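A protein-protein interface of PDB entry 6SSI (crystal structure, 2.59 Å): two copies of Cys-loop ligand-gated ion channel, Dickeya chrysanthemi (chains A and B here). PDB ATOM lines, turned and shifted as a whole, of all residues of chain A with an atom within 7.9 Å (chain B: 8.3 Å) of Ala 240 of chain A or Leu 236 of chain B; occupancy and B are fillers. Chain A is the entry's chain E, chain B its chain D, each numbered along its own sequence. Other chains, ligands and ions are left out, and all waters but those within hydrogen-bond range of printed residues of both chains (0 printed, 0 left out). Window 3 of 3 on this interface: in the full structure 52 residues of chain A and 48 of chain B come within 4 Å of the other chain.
O of Thr 233 of chain A lies within hydrogen-bond range of OG1 of Thr 237 of chain A.
O of Tyr 241 of chain A is in hydrogen-bond range of OG1 of Thr 245 of chain A (3.4 Å).
O of Phe 243 of chain A is in hydrogen-bond range of OG of Ser 246 of chain A.
Among the printed residues, pairs that only touch across the chains: Phe 243 of chain A with Phe 243 of chain B, Tyr 244 of chain A with Ala 242 of chain B, Tyr 244 of chain A with Phe 243 of chain B, Thr 237 of chain A with Leu 236 of chain B, Leu 234 of chain A with Phe 232 of chain B, Ile 211 of chain A with Val 239 of chain B, Tyr 241 of chain A with Tyr 266 of chain B, Ala 240 of chain A with Val 239 of chain B, Ala 240 of chain A with Leu 236 of chain B, Tyr 241 of chain A with Val 239 of chain B, Thr 233 of chain A with Phe 232 of chain B and Leu 236 of chain A with Leu 236 of chain B.
Printed residues of chain B within 4 Å of Leu 234 of chain A: Phe 232 (3.6 Å).
Of the printed residues of chain B, Leu 236 of chain A touches Leu 236 (3.96 Å).
Of chain B, only Leu 236 and Val 239 come within 4 Å of Ala 240 of chain A.
Of chain A, only Leu 236, Thr 237 and Ala 240 come within 4 Å of Leu 236 of chain B.
The nearest residue of chain B that does not touch Ala 240 of chain A is Ala 240 of chain B (5.5 Å).
Of the 18 printed residues of chain A, 9 touch a printed residue of chain B.
Hydrophobic or aromatic side chains of chain B within 4 Å of the printed part of chain A: Phe 232, Leu 236, Val 239, Phe 243 and Tyr 266.
Along chain B the printed residues that touch a printed residue of chain A span positions 232 to 266.
Among the printed residues, 12 pairs touch across the chains.
Among the printed residues, no Asp or Glu carboxylate lies within 4 Å of a Lys or Arg side-chain nitrogen of the other chain.
Thr 233 of chain A touches Phe 232 of chain B, but with the chains exchanged Phe 232 of chain A does not touch Thr 233 of chain B (9.3 Å).
Leu 236 of chain B touches its own counterpart, Leu 236 of chain A.
Ala 240 of chain A touches Leu 236 of chain B, but with the chains exchanged Leu 236 of chain A does not touch Ala 240 of chain B (8.5 Å).
Phe 243 of chain A touches its own counterpart, Phe 243 of chain B.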
ATOM      1  N   ILE A 211     -17.295  26.317 -11.159  1.00  0.00           N
ATOM      2  CA  ILE A 211     -17.943  25.044 -10.815  1.00  0.00           C
ATOM      3  C   ILE A 211     -17.173  24.343  -9.711  1.00  0.00           C
ATOM      4  O   ILE A 211     -17.784  23.937  -8.723  1.00  0.00           O
ATOM      5  CB  ILE A 211     -18.160  24.141 -12.061  1.00  0.00           C
ATOM      6  CG1 ILE A 211     -19.172  24.794 -13.016  1.00  0.00           C
ATOM      7  CG2 ILE A 211     -18.597  22.692 -11.676  1.00  0.00           C
ATOM      8  CD1 ILE A 211     -19.223  24.188 -14.339  1.00  0.00           C
ATOM      9  N   PHE A 232     -23.622  14.477  -4.988  1.00  0.00           N
ATOM     10  CA  PHE A 232     -23.995  13.753  -6.198  1.00  0.00           C
ATOM     11  C   PHE A 232     -24.428  14.691  -7.310  1.00  0.00           C
ATOM     12  O   PHE A 232     -24.106  14.437  -8.472  1.00  0.00           O
ATOM     13  CB  PHE A 232     -25.034  12.669  -5.914  1.00  0.00           C
ATOM     14  CG  PHE A 232     -24.542  11.633  -4.933  1.00  0.00           C
ATOM     15  CD1 PHE A 232     -23.482  10.791  -5.255  1.00  0.00           C
ATOM     16  CD2 PHE A 232     -25.098  11.534  -3.668  1.00  0.00           C
ATOM     17  CE1 PHE A 232     -23.025   9.839  -4.343  1.00  0.00           C
ATOM     18  CE2 PHE A 232     -24.642  10.576  -2.759  1.00  0.00           C
ATOM     19  CZ  PHE A 232     -23.619   9.730  -3.107  1.00  0.00           C
ATOM     20  N   THR A 233     -25.093  15.801  -6.955  1.00  0.00           N
ATOM     21  CA  THR A 233     -25.481  16.833  -7.915  1.00  0.00           C
ATOM     22  C   THR A 233     -24.209  17.515  -8.434  1.00  0.00           C
ATOM     23  O   THR A 233     -24.144  17.893  -9.609  1.00  0.00           O
ATOM     24  CB  THR A 233     -26.495  17.803  -7.292  1.00  0.00           C
ATOM     25  OG1 THR A 233     -27.645  17.057  -6.887  1.00  0.00           O
ATOM     26  CG2 THR A 233     -26.932  18.917  -8.262  1.00  0.00           C
ATOM     27  N   LEU A 234     -23.195  17.641  -7.568  1.00  0.00           N
ATOM     28  CA  LEU A 234     -21.925  18.253  -7.942  1.00  0.00           C
ATOM     29  C   LEU A 234     -21.151  17.337  -8.856  1.00  0.00           C
ATOM     30  O   LEU A 234     -20.655  17.800  -9.884  1.00  0.00           O
ATOM     31  CB  LEU A 234     -21.093  18.660  -6.715  1.00  0.00           C
ATOM     32  CG  LEU A 234     -21.659  19.810  -5.879  1.00  0.00           C
ATOM     33  CD1 LEU A 234     -21.047  19.840  -4.495  1.00  0.00           C
ATOM     34  CD2 LEU A 234     -21.528  21.138  -6.599  1.00  0.00           C
ATOM     35  N   MET A 235     -21.087  16.027  -8.507  1.00  0.00           N
ATOM     36  CA  MET A 235     -20.434  14.988  -9.301  1.00  0.00           C
ATOM     37  C   MET A 235     -21.060  14.957 -10.688  1.00  0.00           C
ATOM     38  O   MET A 235     -20.328  14.918 -11.679  1.00  0.00           O
ATOM     39  CB  MET A 235     -20.547  13.615  -8.626  1.00  0.00           C
ATOM     40  CG  MET A 235     -19.762  12.529  -9.345  1.00  0.00           C
ATOM     41  SD  MET A 235     -17.978  12.583  -9.044  1.00  0.00           S
ATOM     42  CE  MET A 235     -17.922  11.853  -7.420  1.00  0.00           C
ATOM     43  N   LEU A 236     -22.403  15.049 -10.754  1.00  0.00           N
ATOM     44  CA  LEU A 236     -23.154  15.088 -12.004  1.00  0.00           C
ATOM     45  C   LEU A 236     -22.817  16.343 -12.830  1.00  0.00           C
ATOM     46  O   LEU A 236     -22.799  16.267 -14.062  1.00  0.00           O
ATOM     47  CB  LEU A 236     -24.674  14.983 -11.734  1.00  0.00           C
ATOM     48  CG  LEU A 236     -25.606  14.872 -12.959  1.00  0.00           C
ATOM     49  CD1 LEU A 236     -25.268  13.663 -13.818  1.00  0.00           C
ATOM     50  CD2 LEU A 236     -27.058  14.835 -12.544  1.00  0.00           C
ATOM     51  N   THR A 237     -22.528  17.477 -12.167  1.00  0.00           N
ATOM     52  CA  THR A 237     -22.179  18.727 -12.851  1.00  0.00           C
ATOM     53  C   THR A 237     -20.806  18.633 -13.541  1.00  0.00           C
ATOM     54  O   THR A 237     -20.644  19.149 -14.653  1.00  0.00           O
ATOM     55  CB  THR A 237     -22.305  19.929 -11.901  1.00  0.00           C
ATOM     56  OG1 THR A 237     -23.630  19.935 -11.359  1.00  0.00           O
ATOM     57  CG2 THR A 237     -22.017  21.270 -12.597  1.00  0.00           C
ATOM     58  N   VAL A 238     -19.832  17.978 -12.888  1.00  0.00           N
ATOM     59  CA  VAL A 238     -18.490  17.802 -13.447  1.00  0.00           C
ATOM     60  C   VAL A 238     -18.544  16.873 -14.656  1.00  0.00           C
ATOM     61  O   VAL A 238     -17.852  17.123 -15.646  1.00  0.00           O
ATOM     62  CB  VAL A 238     -17.467  17.375 -12.370  1.00  0.00           C
ATOM     63  CG1 VAL A 238     -16.123  16.981 -12.985  1.00  0.00           C
ATOM     64  CG2 VAL A 238     -17.267  18.507 -11.375  1.00  0.00           C
ATOM     65  N   VAL A 239     -19.412  15.840 -14.590  1.00  0.00           N
ATOM     66  CA  VAL A 239     -19.644  14.888 -15.680  1.00  0.00           C
ATOM     67  C   VAL A 239     -20.224  15.642 -16.887  1.00  0.00           C
ATOM     68  O   VAL A 239     -19.708  15.506 -18.000  1.00  0.00           O
ATOM     69  CB  VAL A 239     -20.515  13.673 -15.247  1.00  0.00           C
ATOM     70  CG1 VAL A 239     -20.925  12.827 -16.446  1.00  0.00           C
ATOM     71  CG2 VAL A 239     -19.780  12.803 -14.236  1.00  0.00           C
ATOM     72  N   ALA A 240     -21.255  16.480 -16.649  1.00  0.00           N
ATOM     73  CA  ALA A 240     -21.872  17.297 -17.693  1.00  0.00           C
ATOM     74  C   ALA A 240     -20.846  18.229 -18.306  1.00  0.00           C
ATOM     75  O   ALA A 240     -20.874  18.431 -19.517  1.00  0.00           O
ATOM     76  CB  ALA A 240     -23.032  18.101 -17.130  1.00  0.00           C
ATOM     77  N   TYR A 241     -19.913  18.757 -17.486  1.00  0.00           N
ATOM     78  CA  TYR A 241     -18.875  19.668 -17.955  1.00  0.00           C
ATOM     79  C   TYR A 241     -17.776  18.973 -18.733  1.00  0.00           C
ATOM     80  O   TYR A 241     -17.316  19.516 -19.733  1.00  0.00           O
ATOM     81  CB  TYR A 241     -18.287  20.514 -16.817  1.00  0.00           C
ATOM     82  CG  TYR A 241     -17.681  21.809 -17.323  1.00  0.00           C
ATOM     83  CD1 TYR A 241     -18.469  22.941 -17.516  1.00  0.00           C
ATOM     84  CD2 TYR A 241     -16.338  21.883 -17.681  1.00  0.00           C
ATOM     85  CE1 TYR A 241     -17.925  24.131 -17.993  1.00  0.00           C
ATOM     86  CE2 TYR A 241     -15.782  23.069 -18.164  1.00  0.00           C
ATOM     87  CZ  TYR A 241     -16.584  24.191 -18.317  1.00  0.00           C
ATOM     88  OH  TYR A 241     -16.106  25.379 -18.797  1.00  0.00           O
ATOM     89  N   ALA A 242     -17.355  17.774 -18.286  1.00  0.00           N
ATOM     90  CA  ALA A 242     -16.314  16.979 -18.945  1.00  0.00           C
ATOM     91  C   ALA A 242     -16.718  16.693 -20.382  1.00  0.00           C
ATOM     92  O   ALA A 242     -15.885  16.719 -21.293  1.00  0.00           O
ATOM     93  CB  ALA A 242     -16.103  15.671 -18.201  1.00  0.00           C
ATOM     94  N   PHE A 243     -18.011  16.470 -20.584  1.00  0.00           N
ATOM     95  CA  PHE A 243     -18.533  16.180 -21.894  1.00  0.00           C
ATOM     96  C   PHE A 243     -18.664  17.429 -22.749  1.00  0.00           C
ATOM     97  O   PHE A 243     -18.360  17.358 -23.939  1.00  0.00           O
ATOM     98  CB  PHE A 243     -19.830  15.369 -21.804  1.00  0.00           C
ATOM     99  CG  PHE A 243     -20.934  15.806 -22.730  1.00  0.00           C
ATOM    100  CD1 PHE A 243     -20.784  15.720 -24.114  1.00  0.00           C
ATOM    101  CD2 PHE A 243     -22.112  16.335 -22.224  1.00  0.00           C
ATOM    102  CE1 PHE A 243     -21.767  16.215 -24.962  1.00  0.00           C
ATOM    103  CE2 PHE A 243     -23.121  16.767 -23.078  1.00  0.00           C
ATOM    104  CZ  PHE A 243     -22.959  16.653 -24.435  1.00  0.00           C
ATOM    105  N   TYR A 244     -19.117  18.553 -22.176  1.00  0.00           N
ATOM    106  CA  TYR A 244     -19.239  19.830 -22.887  1.00  0.00           C
ATOM    107  C   TYR A 244     -17.883  20.199 -23.533  1.00  0.00           C
ATOM    108  O   TYR A 244     -17.831  20.665 -24.675  1.00  0.00           O
ATOM    109  CB  TYR A 244     -19.729  20.927 -21.908  1.00  0.00           C
ATOM    110  CG  TYR A 244     -19.443  22.352 -22.336  1.00  0.00           C
ATOM    111  CD1 TYR A 244     -19.947  22.857 -23.531  1.00  0.00           C
ATOM    112  CD2 TYR A 244     -18.659  23.192 -21.555  1.00  0.00           C
ATOM    113  CE1 TYR A 244     -19.668  24.155 -23.943  1.00  0.00           C
ATOM    114  CE2 TYR A 244     -18.370  24.495 -21.960  1.00  0.00           C
ATOM    115  CZ  TYR A 244     -18.876  24.971 -23.157  1.00  0.00           C
ATOM    116  OH  TYR A 244     -18.606  26.252 -23.569  1.00  0.00           O
ATOM    117  N   THR A 245     -16.795  19.951 -22.794  1.00  0.00           N
ATOM    118  CA  THR A 245     -15.443  20.238 -23.239  1.00  0.00           C
ATOM    119  C   THR A 245     -14.973  19.244 -24.271  1.00  0.00           C
ATOM    120  O   THR A 245     -14.568  19.665 -25.350  1.00  0.00           O
ATOM    121  CB  THR A 245     -14.475  20.324 -22.058  1.00  0.00           C
ATOM    122  OG1 THR A 245     -14.428  19.066 -21.391  1.00  0.00           O
ATOM    123  CG2 THR A 245     -14.857  21.386 -21.087  1.00  0.00           C
ATOM    124  N   SER A 246     -15.030  17.935 -23.962  1.00  0.00           N
ATOM    125  CA  SER A 246     -14.589  16.883 -24.881  1.00  0.00           C
ATOM    126  C   SER A 246     -15.265  16.965 -26.258  1.00  0.00           C
ATOM    127  O   SER A 246     -14.641  16.617 -27.253  1.00  0.00           O
ATOM    128  CB  SER A 246     -14.799  15.505 -24.270  1.00  0.00           C
ATOM    129  OG  SER A 246     -16.172  15.151 -24.291  1.00  0.00           O
ATOM    130  N   ILE A 262     -10.527  19.067 -15.031  1.00  0.00           N
ATOM    131  CA  ILE A 262     -11.689  18.182 -14.952  1.00  0.00           C
ATOM    132  C   ILE A 262     -11.405  17.058 -13.961  1.00  0.00           C
ATOM    133  O   ILE A 262     -12.246  16.795 -13.101  1.00  0.00           O
ATOM    134  CB  ILE A 262     -12.134  17.651 -16.339  1.00  0.00           C
ATOM    135  CG1 ILE A 262     -12.527  18.797 -17.302  1.00  0.00           C
ATOM    136  CG2 ILE A 262     -13.237  16.593 -16.221  1.00  0.00           C
ATOM    137  CD1 ILE A 262     -13.856  19.470 -17.057  1.00  0.00           C
ATOM    138  N   TYR A 266     -13.193  16.197 -10.220  1.00  0.00           N
ATOM    139  CA  TYR A 266     -13.657  14.882  -9.768  1.00  0.00           C
ATOM    140  C   TYR A 266     -13.117  14.547  -8.395  1.00  0.00           C
ATOM    141  O   TYR A 266     -13.898  14.192  -7.510  1.00  0.00           O
ATOM    142  CB  TYR A 266     -13.284  13.770 -10.761  1.00  0.00           C
ATOM    143  CG  TYR A 266     -14.171  13.696 -11.983  1.00  0.00           C
ATOM    144  CD1 TYR A 266     -15.503  13.297 -11.881  1.00  0.00           C
ATOM    145  CD2 TYR A 266     -13.656  13.928 -13.255  1.00  0.00           C
ATOM    146  CE1 TYR A 266     -16.315  13.194 -13.010  1.00  0.00           C
ATOM    147  CE2 TYR A 266     -14.458  13.827 -14.390  1.00  0.00           C
ATOM    148  CZ  TYR A 266     -15.786  13.458 -14.263  1.00  0.00           C
ATOM    149  OH  TYR A 266     -16.570  13.343 -15.385  1.00  0.00           O
ATOM    150  N   ILE B 211     -33.862  31.424 -18.838  1.00  0.00           N
ATOM    151  CA  ILE B 211     -33.100  30.619 -17.877  1.00  0.00           C
ATOM    152  C   ILE B 211     -32.392  31.535 -16.892  1.00  0.00           C
ATOM    153  O   ILE B 211     -32.474  31.291 -15.687  1.00  0.00           O
ATOM    154  CB  ILE B 211     -32.126  29.631 -18.564  1.00  0.00           C
ATOM    155  CG1 ILE B 211     -32.910  28.517 -19.276  1.00  0.00           C
ATOM    156  CG2 ILE B 211     -31.083  29.041 -17.569  1.00  0.00           C
ATOM    157  CD1 ILE B 211     -32.088  27.675 -20.218  1.00  0.00           C
ATOM    158  N   GLN B 229     -29.028  24.600  -2.436  1.00  0.00           N
ATOM    159  CA  GLN B 229     -29.206  23.377  -3.215  1.00  0.00           C
ATOM    160  C   GLN B 229     -29.802  23.643  -4.593  1.00  0.00           C
ATOM    161  O   GLN B 229     -29.376  23.011  -5.552  1.00  0.00           O
ATOM    162  CB  GLN B 229     -30.015  22.336  -2.437  1.00  0.00           C
ATOM    163  CG  GLN B 229     -29.276  21.815  -1.203  1.00  0.00           C
ATOM    164  CD  GLN B 229     -30.102  20.854  -0.396  1.00  0.00           C
ATOM    165  OE1 GLN B 229     -31.189  21.174   0.099  1.00  0.00           O
ATOM    166  NE2 GLN B 229     -29.593  19.646  -0.236  1.00  0.00           N
ATOM    167  N   THR B 230     -30.741  24.600  -4.708  1.00  0.00           N
ATOM    168  CA  THR B 230     -31.362  24.980  -5.983  1.00  0.00           C
ATOM    169  C   THR B 230     -30.356  25.661  -6.895  1.00  0.00           C
ATOM    170  O   THR B 230     -30.484  25.543  -8.111  1.00  0.00           O
ATOM    171  CB  THR B 230     -32.613  25.833  -5.733  1.00  0.00           C
ATOM    172  OG1 THR B 230     -33.575  25.031  -5.050  1.00  0.00           O
ATOM    173  CG2 THR B 230     -33.233  26.386  -7.000  1.00  0.00           C
ATOM    174  N   SER B 231     -29.354  26.355  -6.321  1.00  0.00           N
ATOM    175  CA  SER B 231     -28.319  27.023  -7.105  1.00  0.00           C
ATOM    176  C   SER B 231     -27.493  26.027  -7.911  1.00  0.00           C
ATOM    177  O   SER B 231     -27.059  26.368  -9.010  1.00  0.00           O
ATOM    178  CB  SER B 231     -27.422  27.879  -6.221  1.00  0.00           C
ATOM    179  OG  SER B 231     -28.088  29.073  -5.842  1.00  0.00           O
ATOM    180  N   PHE B 232     -27.319  24.792  -7.392  1.00  0.00           N
ATOM    181  CA  PHE B 232     -26.579  23.732  -8.065  1.00  0.00           C
ATOM    182  C   PHE B 232     -27.342  23.203  -9.263  1.00  0.00           C
ATOM    183  O   PHE B 232     -26.729  22.967 -10.306  1.00  0.00           O
ATOM    184  CB  PHE B 232     -26.173  22.614  -7.098  1.00  0.00           C
ATOM    185  CG  PHE B 232     -25.303  23.087  -5.957  1.00  0.00           C
ATOM    186  CD1 PHE B 232     -24.084  23.712  -6.199  1.00  0.00           C
ATOM    187  CD2 PHE B 232     -25.712  22.928  -4.642  1.00  0.00           C
ATOM    188  CE1 PHE B 232     -23.290  24.165  -5.142  1.00  0.00           C
ATOM    189  CE2 PHE B 232     -24.914  23.376  -3.584  1.00  0.00           C
ATOM    190  CZ  PHE B 232     -23.704  23.977  -3.842  1.00  0.00           C
ATOM    191  N   THR B 233     -28.681  23.071  -9.142  1.00  0.00           N
ATOM    192  CA  THR B 233     -29.550  22.649 -10.241  1.00  0.00           C
ATOM    193  C   THR B 233     -29.524  23.712 -11.327  1.00  0.00           C
ATOM    194  O   THR B 233     -29.571  23.372 -12.507  1.00  0.00           O
ATOM    195  CB  THR B 233     -30.965  22.333  -9.731  1.00  0.00           C
ATOM    196  OG1 THR B 233     -30.859  21.281  -8.770  1.00  0.00           O
ATOM    197  CG2 THR B 233     -31.930  21.899 -10.852  1.00  0.00           C
ATOM    198  N   LEU B 234     -29.424  24.992 -10.927  1.00  0.00           N
ATOM    199  CA  LEU B 234     -29.364  26.123 -11.850  1.00  0.00           C
ATOM    200  C   LEU B 234     -28.033  26.135 -12.581  1.00  0.00           C
ATOM    201  O   LEU B 234     -28.017  26.270 -13.805  1.00  0.00           O
ATOM    202  CB  LEU B 234     -29.616  27.459 -11.124  1.00  0.00           C
ATOM    203  CG  LEU B 234     -31.050  27.729 -10.665  1.00  0.00           C
ATOM    204  CD1 LEU B 234     -31.096  28.847  -9.624  1.00  0.00           C
ATOM    205  CD2 LEU B 234     -31.939  28.042 -11.841  1.00  0.00           C
ATOM    206  N   MET B 235     -26.924  25.963 -11.832  1.00  0.00           N
ATOM    207  CA  MET B 235     -25.566  25.866 -12.368  1.00  0.00           C
ATOM    208  C   MET B 235     -25.519  24.714 -13.372  1.00  0.00           C
ATOM    209  O   MET B 235     -24.994  24.895 -14.465  1.00  0.00           O
ATOM    210  CB  MET B 235     -24.547  25.647 -11.235  1.00  0.00           C
ATOM    211  CG  MET B 235     -23.109  25.665 -11.697  1.00  0.00           C
ATOM    212  SD  MET B 235     -22.466  27.341 -11.882  1.00  0.00           S
ATOM    213  CE  MET B 235     -22.027  27.694 -10.209  1.00  0.00           C
ATOM    214  N   LEU B 236     -26.130  23.564 -13.026  1.00  0.00           N
ATOM    215  CA  LEU B 236     -26.219  22.399 -13.899  1.00  0.00           C
ATOM    216  C   LEU B 236     -27.033  22.695 -15.177  1.00  0.00           C
ATOM    217  O   LEU B 236     -26.728  22.143 -16.238  1.00  0.00           O
ATOM    218  CB  LEU B 236     -26.805  21.196 -13.131  1.00  0.00           C
ATOM    219  CG  LEU B 236     -26.836  19.844 -13.852  1.00  0.00           C
ATOM    220  CD1 LEU B 236     -25.465  19.472 -14.449  1.00  0.00           C
ATOM    221  CD2 LEU B 236     -27.337  18.762 -12.939  1.00  0.00           C
ATOM    222  N   THR B 237     -28.041  23.580 -15.084  1.00  0.00           N
ATOM    223  CA  THR B 237     -28.873  23.973 -16.225  1.00  0.00           C
ATOM    224  C   THR B 237     -28.081  24.824 -17.197  1.00  0.00           C
ATOM    225  O   THR B 237     -28.252  24.684 -18.413  1.00  0.00           O
ATOM    226  CB  THR B 237     -30.178  24.630 -15.758  1.00  0.00           C
ATOM    227  OG1 THR B 237     -30.861  23.684 -14.937  1.00  0.00           O
ATOM    228  CG2 THR B 237     -31.094  25.059 -16.927  1.00  0.00           C
ATOM    229  N   VAL B 238     -27.223  25.706 -16.664  1.00  0.00           N
ATOM    230  CA  VAL B 238     -26.401  26.571 -17.499  1.00  0.00           C
ATOM    231  C   VAL B 238     -25.387  25.748 -18.254  1.00  0.00           C
ATOM    232  O   VAL B 238     -25.156  26.032 -19.421  1.00  0.00           O
ATOM    233  CB  VAL B 238     -25.790  27.760 -16.740  1.00  0.00           C
ATOM    234  CG1 VAL B 238     -24.783  28.523 -17.608  1.00  0.00           C
ATOM    235  CG2 VAL B 238     -26.895  28.694 -16.288  1.00  0.00           C
ATOM    236  N   VAL B 239     -24.834  24.703 -17.612  1.00  0.00           N
ATOM    237  CA  VAL B 239     -23.868  23.796 -18.225  1.00  0.00           C
ATOM    238  C   VAL B 239     -24.556  23.037 -19.345  1.00  0.00           C
ATOM    239  O   VAL B 239     -24.010  22.948 -20.445  1.00  0.00           O
ATOM    240  CB  VAL B 239     -23.200  22.853 -17.184  1.00  0.00           C
ATOM    241  CG1 VAL B 239     -22.281  21.830 -17.849  1.00  0.00           C
ATOM    242  CG2 VAL B 239     -22.425  23.648 -16.144  1.00  0.00           C
ATOM    243  N   ALA B 240     -25.768  22.516 -19.070  1.00  0.00           N
ATOM    244  CA  ALA B 240     -26.567  21.771 -20.040  1.00  0.00           C
ATOM    245  C   ALA B 240     -26.893  22.663 -21.228  1.00  0.00           C
ATOM    246  O   ALA B 240     -26.867  22.200 -22.367  1.00  0.00           O
ATOM    247  CB  ALA B 240     -27.841  21.252 -19.394  1.00  0.00           C
ATOM    248  N   TYR B 241     -27.129  23.955 -20.973  1.00  0.00           N
ATOM    249  CA  TYR B 241     -27.410  24.914 -22.028  1.00  0.00           C
ATOM    250  C   TYR B 241     -26.155  25.326 -22.790  1.00  0.00           C
ATOM    251  O   TYR B 241     -26.241  25.529 -24.001  1.00  0.00           O
ATOM    252  CB  TYR B 241     -28.141  26.150 -21.485  1.00  0.00           C
ATOM    253  CG  TYR B 241     -28.867  26.914 -22.569  1.00  0.00           C
ATOM    254  CD1 TYR B 241     -30.145  26.542 -22.975  1.00  0.00           C
ATOM    255  CD2 TYR B 241     -28.262  27.986 -23.219  1.00  0.00           C
ATOM    256  CE1 TYR B 241     -30.816  27.233 -23.977  1.00  0.00           C
ATOM    257  CE2 TYR B 241     -28.924  28.686 -24.225  1.00  0.00           C
ATOM    258  CZ  TYR B 241     -30.199  28.296 -24.606  1.00  0.00           C
ATOM    259  OH  TYR B 241     -30.881  28.924 -25.607  1.00  0.00           O
ATOM    260  N   ALA B 242     -25.007  25.475 -22.090  1.00  0.00           N
ATOM    261  CA  ALA B 242     -23.720  25.910 -22.641  1.00  0.00           C
ATOM    262  C   ALA B 242     -23.254  24.962 -23.718  1.00  0.00           C
ATOM    263  O   ALA B 242     -22.677  25.386 -24.720  1.00  0.00           O
ATOM    264  CB  ALA B 242     -22.677  25.997 -21.539  1.00  0.00           C
ATOM    265  N   PHE B 243     -23.530  23.676 -23.518  1.00  0.00           N
ATOM    266  CA  PHE B 243     -23.183  22.659 -24.473  1.00  0.00           C
ATOM    267  C   PHE B 243     -24.166  22.646 -25.640  1.00  0.00           C
ATOM    268  O   PHE B 243     -23.721  22.612 -26.785  1.00  0.00           O
ATOM    269  CB  PHE B 243     -23.061  21.274 -23.809  1.00  0.00           C
ATOM    270  CG  PHE B 243     -23.296  20.201 -24.831  1.00  0.00           C
ATOM    271  CD1 PHE B 243     -22.310  19.877 -25.763  1.00  0.00           C
ATOM    272  CD2 PHE B 243     -24.555  19.637 -24.982  1.00  0.00           C
ATOM    273  CE1 PHE B 243     -22.574  18.986 -26.798  1.00  0.00           C
ATOM    274  CE2 PHE B 243     -24.813  18.760 -26.016  1.00  0.00           C
ATOM    275  CZ  PHE B 243     -23.817  18.416 -26.904  1.00  0.00           C
ATOM    276  N   TYR B 266     -23.297  32.004 -15.753  1.00  0.00           N
ATOM    277  CA  TYR B 266     -22.404  31.356 -14.788  1.00  0.00           C
ATOM    278  C   TYR B 266     -22.121  32.256 -13.606  1.00  0.00           C
ATOM    279  O   TYR B 266     -22.222  31.805 -12.466  1.00  0.00           O
ATOM    280  CB  TYR B 266     -21.085  30.933 -15.438  1.00  0.00           C
ATOM    281  CG  TYR B 266     -21.156  29.627 -16.185  1.00  0.00           C
ATOM    282  CD1 TYR B 266     -21.394  28.429 -15.514  1.00  0.00           C
ATOM    283  CD2 TYR B 266     -20.889  29.569 -17.549  1.00  0.00           C
ATOM    284  CE1 TYR B 266     -21.429  27.214 -16.193  1.00  0.00           C
ATOM    285  CE2 TYR B 266     -20.896  28.357 -18.234  1.00  0.00           C
ATOM    286  CZ  TYR B 266     -21.173  27.184 -17.553  1.00  0.00           C
ATOM    287  OH  TYR B 266     -21.193  25.990 -18.226  1.00  0.00           O
ATOM    288  N   ILE B 269     -25.302  32.959 -11.282  1.00  0.00           N
ATOM    289  CA  ILE B 269     -25.549  31.821 -10.396  1.00  0.00           C
ATOM    290  C   ILE B 269     -24.458  31.739  -9.334  1.00  0.00           C
ATOM    291  O   ILE B 269     -24.774  31.502  -8.168  1.00  0.00           O
ATOM    292  CB  ILE B 269     -25.755  30.495 -11.183  1.00  0.00           C
ATOM    293  CG1 ILE B 269     -27.028  30.596 -12.039  1.00  0.00           C
ATOM    294  CG2 ILE B 269     -25.797  29.246 -10.264  1.00  0.00           C
ATOM    295  CD1 ILE B 269     -27.189  29.555 -13.012  1.00  0.00           C
